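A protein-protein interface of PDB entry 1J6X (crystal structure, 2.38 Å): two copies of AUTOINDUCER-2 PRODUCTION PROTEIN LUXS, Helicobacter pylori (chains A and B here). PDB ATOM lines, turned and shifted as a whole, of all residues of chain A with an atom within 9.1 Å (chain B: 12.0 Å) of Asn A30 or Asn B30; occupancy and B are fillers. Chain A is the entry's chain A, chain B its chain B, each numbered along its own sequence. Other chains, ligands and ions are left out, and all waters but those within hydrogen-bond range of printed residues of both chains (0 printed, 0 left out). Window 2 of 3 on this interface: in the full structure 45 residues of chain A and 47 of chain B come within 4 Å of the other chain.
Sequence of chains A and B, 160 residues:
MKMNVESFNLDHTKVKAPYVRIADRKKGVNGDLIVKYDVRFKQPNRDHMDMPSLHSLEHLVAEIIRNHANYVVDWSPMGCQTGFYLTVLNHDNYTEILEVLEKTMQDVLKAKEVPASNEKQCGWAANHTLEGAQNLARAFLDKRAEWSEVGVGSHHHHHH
O of Lys B26 lies within hydrogen-bond range of N of Ile B34 (2.6 Å).
The side-chain carboxylate (OD1) of Asp B32 is in hydrogen-bond range of the side-chain amide nitrogen (ND2) of Asn B90 (3.0 Å).
The backbone carbonyl oxygen (O) of Leu B33 lies within hydrogen-bond range of the backbone NH (N) of Asn B90 (2.7 Å).
N of Asn A90 is in hydrogen-bond range of O of Leu A33.
The backbone carbonyl oxygen of Gly B31 sits at hydrogen-bond distance from the side-chain amino group of Lys B27, at 3.3 Å.
NZ of Lys A27 lies within hydrogen-bond range of O of Gly A31 (3.3 Å).
Gly A28 touches Leu B89, but with the chains exchanged Leu A89 does not touch Gly B28 (4.3 Å).
Val A29 touches Asp B32, and with the chains exchanged Asp A32 touches Val B29.
Val A29 touches Asn B90, and with the chains exchanged Asn A90 touches Val B29.
Asp B32 touches its own counterpart, Asp A32.
10 positions are printed for both chains.
Of the 19 pairs that touch across the chains among the printed residues, 17 have their exchanged pair printed and touching as well.
Of the 14 printed residues of chain B, 8 touch a printed residue of chain A.
Printed residues of chain B that touch a printed residue of chain A: Gly B28, Val B29, Asn B30, Gly B31, Asp B32, Ile B34, Leu B89 and Asn B90.
Hydrophobic or aromatic side chains of chain B within 4 Å of the printed part of chain A: Val B29, Ile B34 and Leu B89.
Hydrophobic or aromatic side chains of chain A within 4 Å of the printed part of chain B: Val A29, Ile A34 and Leu A89.
Among the printed residues, 19 pairs touch across the chains.
Among the printed residues, no Asp or Glu carboxylate lies within 4 Å of a Lys or Arg side-chain nitrogen of the other chain.
Among the printed residues, pairs that only touch across the chains: Gly A28 with Asp B32 (3.0 Å), Asn A30 with Asn B30 (3.1 Å), Asp A32 with Gly B28 (3.2 Å), Gly A28 with Asn B90 (3.3 Å), Gly A28 with Leu B89 (3.4 Å), Asp A32 with Val B29 (3.5 Å), Leu A89 with Ile B34 (3.5 Å), Ile A34 with Leu B89 (3.7 Å), Gly A31 with Asn B30 (3.7 Å), Asn A90 with Val B29 (3.8 Å), Ile A34 with Ile B34 (3.8 Å) and Asn A30 with Gly B31 (3.9 Å).
The side-chain carboxylate (OD1) of Asp A32 lies within hydrogen-bond range of the side-chain amide nitrogen (ND2) of Asn B30 (2.9 Å).
N of Asp B32 is in hydrogen-bond range of OD2 of Asp A32 (3.0 Å).
The backbone NH (N) of Gly B31 is in hydrogen-bond range of the side-chain carboxylate (OD2) of Asp A32.
The backbone NH (N) of Gly A31 lies within hydrogen-bond range of the side-chain carboxylate (OD2) of Asp B32, 3.2 Å away.
The side-chain amide oxygen of Asn B90 is in hydrogen-bond range of the backbone NH of Val A29 (3.0 Å).
The side-chain carboxylate of Asp B32 lies within hydrogen-bond range of the backbone NH of Asn A30.
N of Val A29 lies within hydrogen-bond range of OD1 of Asp B32, at 3.2 Å.
Printed residues of chain B within 4 Å of Gly A28: Asp B32, Leu B89 and Asn B90.
Val A29 touches just these residues of chain B: Asp B32 and Asn B90.
Of the printed residues of chain B, Asn A30 touches Asn B30 (3.1 Å), Gly B31 (3.9 Å) and Asp B32 (2.8 Å).
Asp A32 touches five residues of chain B.
Of the printed residues of chain B, Leu A89 touches Ile B34.
Printed residues of chain B within 4 Å of Asn A90: Val B29 (3.8 Å).
Of the printed residues of chain A, Gly B28 touches Asp A32 (3.2 Å).
Val B29 touches just these residues of chain A: Asp A32 and Asn A90.
Printed residues of chain A within 4 Å of Asn B30: Asn A30, Gly A31 and Asp A32.
Gly B31 touches two residues of chain A.
Leu B33 touches none of the printed residues of chain A.
Of the printed residues of chain A, Leu B89 touches Gly A28 (3.4 Å) and Ile A34 (3.7 Å).
Asp B92 touches none of the printed residues of chain A.
The nearest residue of chain A that does not touch Asn B30 is Asn A90 (4.2 Å).
The nearest printed residue of chain B that does not touch Asn A90 is Asn B30 (4.2 Å).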
ATOM      1  N   LYS A  27     -10.377 -23.936 -13.591  1.00  0.00           N
ATOM      2  CA  LYS A  27      -9.631 -23.803 -12.342  1.00  0.00           C
ATOM      3  C   LYS A  27      -8.179 -23.435 -12.599  1.00  0.00           C
ATOM      4  O   LYS A  27      -7.485 -24.098 -13.364  1.00  0.00           O
ATOM      5  CB  LYS A  27      -9.699 -25.104 -11.525  1.00  0.00           C
ATOM      6  CG  LYS A  27      -8.991 -25.022 -10.163  1.00  0.00           C
ATOM      7  CD  LYS A  27      -8.963 -26.371  -9.444  1.00  0.00           C
ATOM      8  CE  LYS A  27     -10.361 -26.844  -9.076  1.00  0.00           C
ATOM      9  NZ  LYS A  27     -11.003 -25.951  -8.072  1.00  0.00           N
ATOM     10  N   GLY A  28      -7.740 -22.361 -11.957  1.00  0.00           N
ATOM     11  CA  GLY A  28      -6.374 -21.911 -12.109  1.00  0.00           C
ATOM     12  C   GLY A  28      -5.396 -22.954 -11.604  1.00  0.00           C
ATOM     13  O   GLY A  28      -5.795 -23.951 -10.992  1.00  0.00           O
ATOM     14  N   VAL A  29      -4.113 -22.722 -11.850  1.00  0.00           N
ATOM     15  CA  VAL A  29      -3.096 -23.664 -11.422  1.00  0.00           C
ATOM     16  C   VAL A  29      -2.975 -23.664  -9.894  1.00  0.00           C
ATOM     17  O   VAL A  29      -2.534 -24.647  -9.308  1.00  0.00           O
ATOM     18  CB  VAL A  29      -1.721 -23.340 -12.079  1.00  0.00           C
ATOM     19  CG1 VAL A  29      -1.105 -22.084 -11.460  1.00  0.00           C
ATOM     20  CG2 VAL A  29      -0.788 -24.522 -11.921  1.00  0.00           C
ATOM     21  N   ASN A  30      -3.393 -22.572  -9.254  1.00  0.00           N
ATOM     22  CA  ASN A  30      -3.328 -22.462  -7.797  1.00  0.00           C
ATOM     23  C   ASN A  30      -4.592 -22.898  -7.047  1.00  0.00           C
ATOM     24  O   ASN A  30      -4.627 -22.841  -5.817  1.00  0.00           O
ATOM     25  CB  ASN A  30      -2.999 -21.029  -7.385  1.00  0.00           C
ATOM     26  CG  ASN A  30      -1.575 -20.638  -7.714  1.00  0.00           C
ATOM     27  OD1 ASN A  30      -0.617 -21.188  -7.160  1.00  0.00           O
ATOM     28  ND2 ASN A  30      -1.427 -19.680  -8.620  1.00  0.00           N
ATOM     29  N   GLY A  31      -5.632 -23.307  -7.768  1.00  0.00           N
ATOM     30  CA  GLY A  31      -6.840 -23.753  -7.089  1.00  0.00           C
ATOM     31  C   GLY A  31      -8.090 -22.908  -7.246  1.00  0.00           C
ATOM     32  O   GLY A  31      -9.191 -23.399  -6.997  1.00  0.00           O
ATOM     33  N   ASP A  32      -7.937 -21.655  -7.670  1.00  0.00           N
ATOM     34  CA  ASP A  32      -9.077 -20.763  -7.843  1.00  0.00           C
ATOM     35  C   ASP A  32     -10.088 -21.230  -8.888  1.00  0.00           C
ATOM     36  O   ASP A  32      -9.721 -21.602 -10.005  1.00  0.00           O
ATOM     37  CB  ASP A  32      -8.596 -19.354  -8.172  1.00  0.00           C
ATOM     38  CG  ASP A  32      -8.098 -18.617  -6.942  1.00  0.00           C
ATOM     39  OD1 ASP A  32      -8.787 -18.674  -5.890  1.00  0.00           O
ATOM     40  OD2 ASP A  32      -7.029 -17.969  -7.026  1.00  0.00           O
ATOM     41  N   LEU A  33     -11.366 -21.196  -8.503  1.00  0.00           N
ATOM     42  CA  LEU A  33     -12.460 -21.641  -9.362  1.00  0.00           C
ATOM     43  C   LEU A  33     -13.165 -20.508 -10.102  1.00  0.00           C
ATOM     44  O   LEU A  33     -13.260 -19.384  -9.626  1.00  0.00           O
ATOM     45  CB  LEU A  33     -13.491 -22.432  -8.535  1.00  0.00           C
ATOM     46  CG  LEU A  33     -14.694 -23.109  -9.228  1.00  0.00           C
ATOM     47  CD1 LEU A  33     -14.238 -24.041 -10.319  1.00  0.00           C
ATOM     48  CD2 LEU A  33     -15.488 -23.899  -8.212  1.00  0.00           C
ATOM     49  N   ILE A  34     -13.654 -20.827 -11.286  1.00  0.00           N
ATOM     50  CA  ILE A  34     -14.378 -19.869 -12.101  1.00  0.00           C
ATOM     51  C   ILE A  34     -15.548 -20.659 -12.681  1.00  0.00           C
ATOM     52  O   ILE A  34     -15.348 -21.683 -13.338  1.00  0.00           O
ATOM     53  CB  ILE A  34     -13.483 -19.328 -13.262  1.00  0.00           C
ATOM     54  CG1 ILE A  34     -12.268 -18.588 -12.683  1.00  0.00           C
ATOM     55  CG2 ILE A  34     -14.296 -18.420 -14.194  1.00  0.00           C
ATOM     56  CD1 ILE A  34     -11.212 -18.264 -13.725  1.00  0.00           C
ATOM     57  N   LEU A  89     -16.285 -16.075  -9.272  1.00  0.00           N
ATOM     58  CA  LEU A  89     -14.984 -16.504  -8.761  1.00  0.00           C
ATOM     59  C   LEU A  89     -15.114 -17.144  -7.373  1.00  0.00           C
ATOM     60  O   LEU A  89     -15.746 -16.584  -6.476  1.00  0.00           O
ATOM     61  CB  LEU A  89     -14.048 -15.291  -8.678  1.00  0.00           C
ATOM     62  CG  LEU A  89     -12.644 -15.502  -8.111  1.00  0.00           C
ATOM     63  CD1 LEU A  89     -11.857 -16.433  -9.018  1.00  0.00           C
ATOM     64  CD2 LEU A  89     -11.948 -14.161  -7.979  1.00  0.00           C
ATOM     65  N   ASN A  90     -14.510 -18.316  -7.205  1.00  0.00           N
ATOM     66  CA  ASN A  90     -14.550 -19.019  -5.928  1.00  0.00           C
ATOM     67  C   ASN A  90     -15.930 -19.069  -5.279  1.00  0.00           C
ATOM     68  O   ASN A  90     -16.080 -18.782  -4.087  1.00  0.00           O
ATOM     69  CB  ASN A  90     -13.560 -18.394  -4.938  1.00  0.00           C
ATOM     70  CG  ASN A  90     -12.132 -18.510  -5.401  1.00  0.00           C
ATOM     71  OD1 ASN A  90     -11.693 -19.576  -5.842  1.00  0.00           O
ATOM     72  ND2 ASN A  90     -11.392 -17.416  -5.304  1.00  0.00           N
ATOM     73  N   LYS B  26      -7.813  -9.290 -11.203  1.00  0.00           N
ATOM     74  CA  LYS B  26      -8.338  -9.851  -9.980  1.00  0.00           C
ATOM     75  C   LYS B  26      -7.421 -11.009  -9.663  1.00  0.00           C
ATOM     76  O   LYS B  26      -7.063 -11.792 -10.541  1.00  0.00           O
ATOM     77  CB  LYS B  26      -9.757 -10.407 -10.170  1.00  0.00           C
ATOM     78  CG  LYS B  26     -10.852  -9.423 -10.567  1.00  0.00           C
ATOM     79  CD  LYS B  26     -12.216 -10.124 -10.440  1.00  0.00           C
ATOM     80  CE  LYS B  26     -13.367  -9.338 -11.076  1.00  0.00           C
ATOM     81  NZ  LYS B  26     -13.351  -9.373 -12.575  1.00  0.00           N
ATOM     82  N   LYS B  27      -7.027 -11.112  -8.407  1.00  0.00           N
ATOM     83  CA  LYS B  27      -6.190 -12.215  -7.996  1.00  0.00           C
ATOM     84  C   LYS B  27      -7.079 -12.975  -7.031  1.00  0.00           C
ATOM     85  O   LYS B  27      -7.641 -12.386  -6.117  1.00  0.00           O
ATOM     86  CB  LYS B  27      -4.939 -11.689  -7.300  1.00  0.00           C
ATOM     87  CG  LYS B  27      -4.048 -12.766  -6.736  1.00  0.00           C
ATOM     88  CD  LYS B  27      -2.758 -12.176  -6.190  1.00  0.00           C
ATOM     89  CE  LYS B  27      -1.852 -11.715  -7.328  1.00  0.00           C
ATOM     90  NZ  LYS B  27      -1.467 -12.856  -8.217  1.00  0.00           N
ATOM     91  N   GLY B  28      -7.248 -14.269  -7.250  1.00  0.00           N
ATOM     92  CA  GLY B  28      -8.090 -15.041  -6.354  1.00  0.00           C
ATOM     93  C   GLY B  28      -7.446 -15.232  -4.989  1.00  0.00           C
ATOM     94  O   GLY B  28      -6.270 -14.913  -4.805  1.00  0.00           O
ATOM     95  N   VAL B  29      -8.213 -15.752  -4.033  1.00  0.00           N
ATOM     96  CA  VAL B  29      -7.707 -15.998  -2.687  1.00  0.00           C
ATOM     97  C   VAL B  29      -6.499 -16.938  -2.756  1.00  0.00           C
ATOM     98  O   VAL B  29      -5.576 -16.825  -1.960  1.00  0.00           O
ATOM     99  CB  VAL B  29      -8.798 -16.633  -1.773  1.00  0.00           C
ATOM    100  CG1 VAL B  29      -9.104 -18.055  -2.219  1.00  0.00           C
ATOM    101  CG2 VAL B  29      -8.326 -16.626  -0.324  1.00  0.00           C
ATOM    102  N   ASN B  30      -6.509 -17.857  -3.720  1.00  0.00           N
ATOM    103  CA  ASN B  30      -5.412 -18.811  -3.905  1.00  0.00           C
ATOM    104  C   ASN B  30      -4.235 -18.283  -4.734  1.00  0.00           C
ATOM    105  O   ASN B  30      -3.278 -19.017  -5.011  1.00  0.00           O
ATOM    106  CB  ASN B  30      -5.934 -20.076  -4.561  1.00  0.00           C
ATOM    107  CG  ASN B  30      -6.892 -20.817  -3.677  1.00  0.00           C
ATOM    108  OD1 ASN B  30      -6.509 -21.316  -2.612  1.00  0.00           O
ATOM    109  ND2 ASN B  30      -8.151 -20.893  -4.098  1.00  0.00           N
ATOM    110  N   GLY B  31      -4.305 -17.024  -5.149  1.00  0.00           N
ATOM    111  CA  GLY B  31      -3.209 -16.479  -5.925  1.00  0.00           C
ATOM    112  C   GLY B  31      -3.331 -16.528  -7.439  1.00  0.00           C
ATOM    113  O   GLY B  31      -2.495 -15.943  -8.127  1.00  0.00           O
ATOM    114  N   ASP B  32      -4.326 -17.227  -7.976  1.00  0.00           N
ATOM    115  CA  ASP B  32      -4.484 -17.261  -9.421  1.00  0.00           C
ATOM    116  C   ASP B  32      -4.902 -15.860  -9.886  1.00  0.00           C
ATOM    117  O   ASP B  32      -5.683 -15.162  -9.230  1.00  0.00           O
ATOM    118  CB  ASP B  32      -5.531 -18.290  -9.845  1.00  0.00           C
ATOM    119  CG  ASP B  32      -4.995 -19.722  -9.848  1.00  0.00           C
ATOM    120  OD1 ASP B  32      -3.820 -19.947 -10.227  1.00  0.00           O
ATOM    121  OD2 ASP B  32      -5.763 -20.640  -9.493  1.00  0.00           O
ATOM    122  N   LEU B  33      -4.372 -15.440 -11.020  1.00  0.00           N
ATOM    123  CA  LEU B  33      -4.683 -14.118 -11.536  1.00  0.00           C
ATOM    124  C   LEU B  33      -5.671 -14.165 -12.705  1.00  0.00           C
ATOM    125  O   LEU B  33      -5.533 -14.970 -13.617  1.00  0.00           O
ATOM    126  CB  LEU B  33      -3.375 -13.440 -11.968  1.00  0.00           C
ATOM    127  CG  LEU B  33      -3.355 -12.015 -12.519  1.00  0.00           C
ATOM    128  CD1 LEU B  33      -3.684 -11.000 -11.448  1.00  0.00           C
ATOM    129  CD2 LEU B  33      -1.974 -11.751 -13.079  1.00  0.00           C
ATOM    130  N   ILE B  34      -6.693 -13.320 -12.650  1.00  0.00           N
ATOM    131  CA  ILE B  34      -7.671 -13.219 -13.734  1.00  0.00           C
ATOM    132  C   ILE B  34      -7.505 -11.798 -14.270  1.00  0.00           C
ATOM    133  O   ILE B  34      -7.541 -10.837 -13.510  1.00  0.00           O
ATOM    134  CB  ILE B  34      -9.120 -13.368 -13.242  1.00  0.00           C
ATOM    135  CG1 ILE B  34      -9.322 -14.736 -12.594  1.00  0.00           C
ATOM    136  CG2 ILE B  34     -10.078 -13.213 -14.411  1.00  0.00           C
ATOM    137  CD1 ILE B  34     -10.713 -14.915 -11.983  1.00  0.00           C
ATOM    138  N   VAL B  88      -8.800 -13.628 -19.356  1.00  0.00           N
ATOM    139  CA  VAL B  88      -7.807 -14.698 -19.301  1.00  0.00           C
ATOM    140  C   VAL B  88      -7.511 -15.052 -17.835  1.00  0.00           C
ATOM    141  O   VAL B  88      -7.855 -14.308 -16.925  1.00  0.00           O
ATOM    142  CB  VAL B  88      -6.500 -14.303 -20.042  1.00  0.00           C
ATOM    143  CG1 VAL B  88      -6.784 -14.144 -21.539  1.00  0.00           C
ATOM    144  CG2 VAL B  88      -5.929 -13.005 -19.467  1.00  0.00           C
ATOM    145  N   LEU B  89      -6.899 -16.207 -17.616  1.00  0.00           N
ATOM    146  CA  LEU B  89      -6.559 -16.672 -16.273  1.00  0.00           C
ATOM    147  C   LEU B  89      -5.101 -17.119 -16.267  1.00  0.00           C
ATOM    148  O   LEU B  89      -4.667 -17.818 -17.182  1.00  0.00           O
ATOM    149  CB  LEU B  89      -7.444 -17.856 -15.882  1.00  0.00           C
ATOM    150  CG  LEU B  89      -6.954 -18.678 -14.682  1.00  0.00           C
ATOM    151  CD1 LEU B  89      -7.543 -18.124 -13.385  1.00  0.00           C
ATOM    152  CD2 LEU B  89      -7.378 -20.129 -14.864  1.00  0.00           C
ATOM    153  N   ASN B  90      -4.355 -16.714 -15.245  1.00  0.00           N
ATOM    154  CA  ASN B  90      -2.949 -17.081 -15.120  1.00  0.00           C
ATOM    155  C   ASN B  90      -2.055 -16.660 -16.308  1.00  0.00           C
ATOM    156  O   ASN B  90      -1.200 -17.432 -16.761  1.00  0.00           O
ATOM    157  CB  ASN B  90      -2.824 -18.598 -14.869  1.00  0.00           C
ATOM    158  CG  ASN B  90      -3.323 -19.010 -13.474  1.00  0.00           C
ATOM    159  OD1 ASN B  90      -3.979 -20.052 -13.306  1.00  0.00           O
ATOM    160  ND2 ASN B  90      -3.011 -18.197 -12.473  1.00  0.00           N
ATOM    161  N   HIS B  91      -2.264 -15.439 -16.803  1.00  0.00           N
ATOM    162  CA  HIS B  91      -1.470 -14.875 -17.896  1.00  0.00           C
ATOM    163  C   HIS B  91      -1.405 -13.382 -17.669  1.00  0.00           C
ATOM    164  O   HIS B  91      -2.427 -12.742 -17.395  1.00  0.00           O
ATOM    165  CB  HIS B  91      -2.096 -15.183 -19.255  1.00  0.00           C
ATOM    166  CG  HIS B  91      -1.294 -14.681 -20.411  1.00  0.00           C
ATOM    167  ND1 HIS B  91      -1.334 -13.367 -20.823  1.00  0.00           N
ATOM    168  CD2 HIS B  91      -0.382 -15.297 -21.203  1.00  0.00           C
ATOM    169  CE1 HIS B  91      -0.481 -13.194 -21.818  1.00  0.00           C
ATOM    170  NE2 HIS B  91       0.110 -14.350 -22.068  1.00  0.00           N
ATOM    171  N   ASP B  92      -0.209 -12.811 -17.776  1.00  0.00           N
ATOM    172  CA  ASP B  92      -0.100 -11.404 -17.498  1.00  0.00           C
ATOM    173  C   ASP B  92       0.965 -10.643 -18.299  1.00  0.00           C
ATOM    174  O   ASP B  92       1.645  -9.789 -17.735  1.00  0.00           O
ATOM    175  CB  ASP B  92       0.124 -11.277 -16.004  1.00  0.00           C
ATOM    176  CG  ASP B  92       0.014  -9.865 -15.499  1.00  0.00           C
ATOM    177  OD1 ASP B  92      -0.990  -9.190 -15.828  1.00  0.00           O
ATOM    178  OD2 ASP B  92       0.905  -9.459 -14.727  1.00  0.00           O
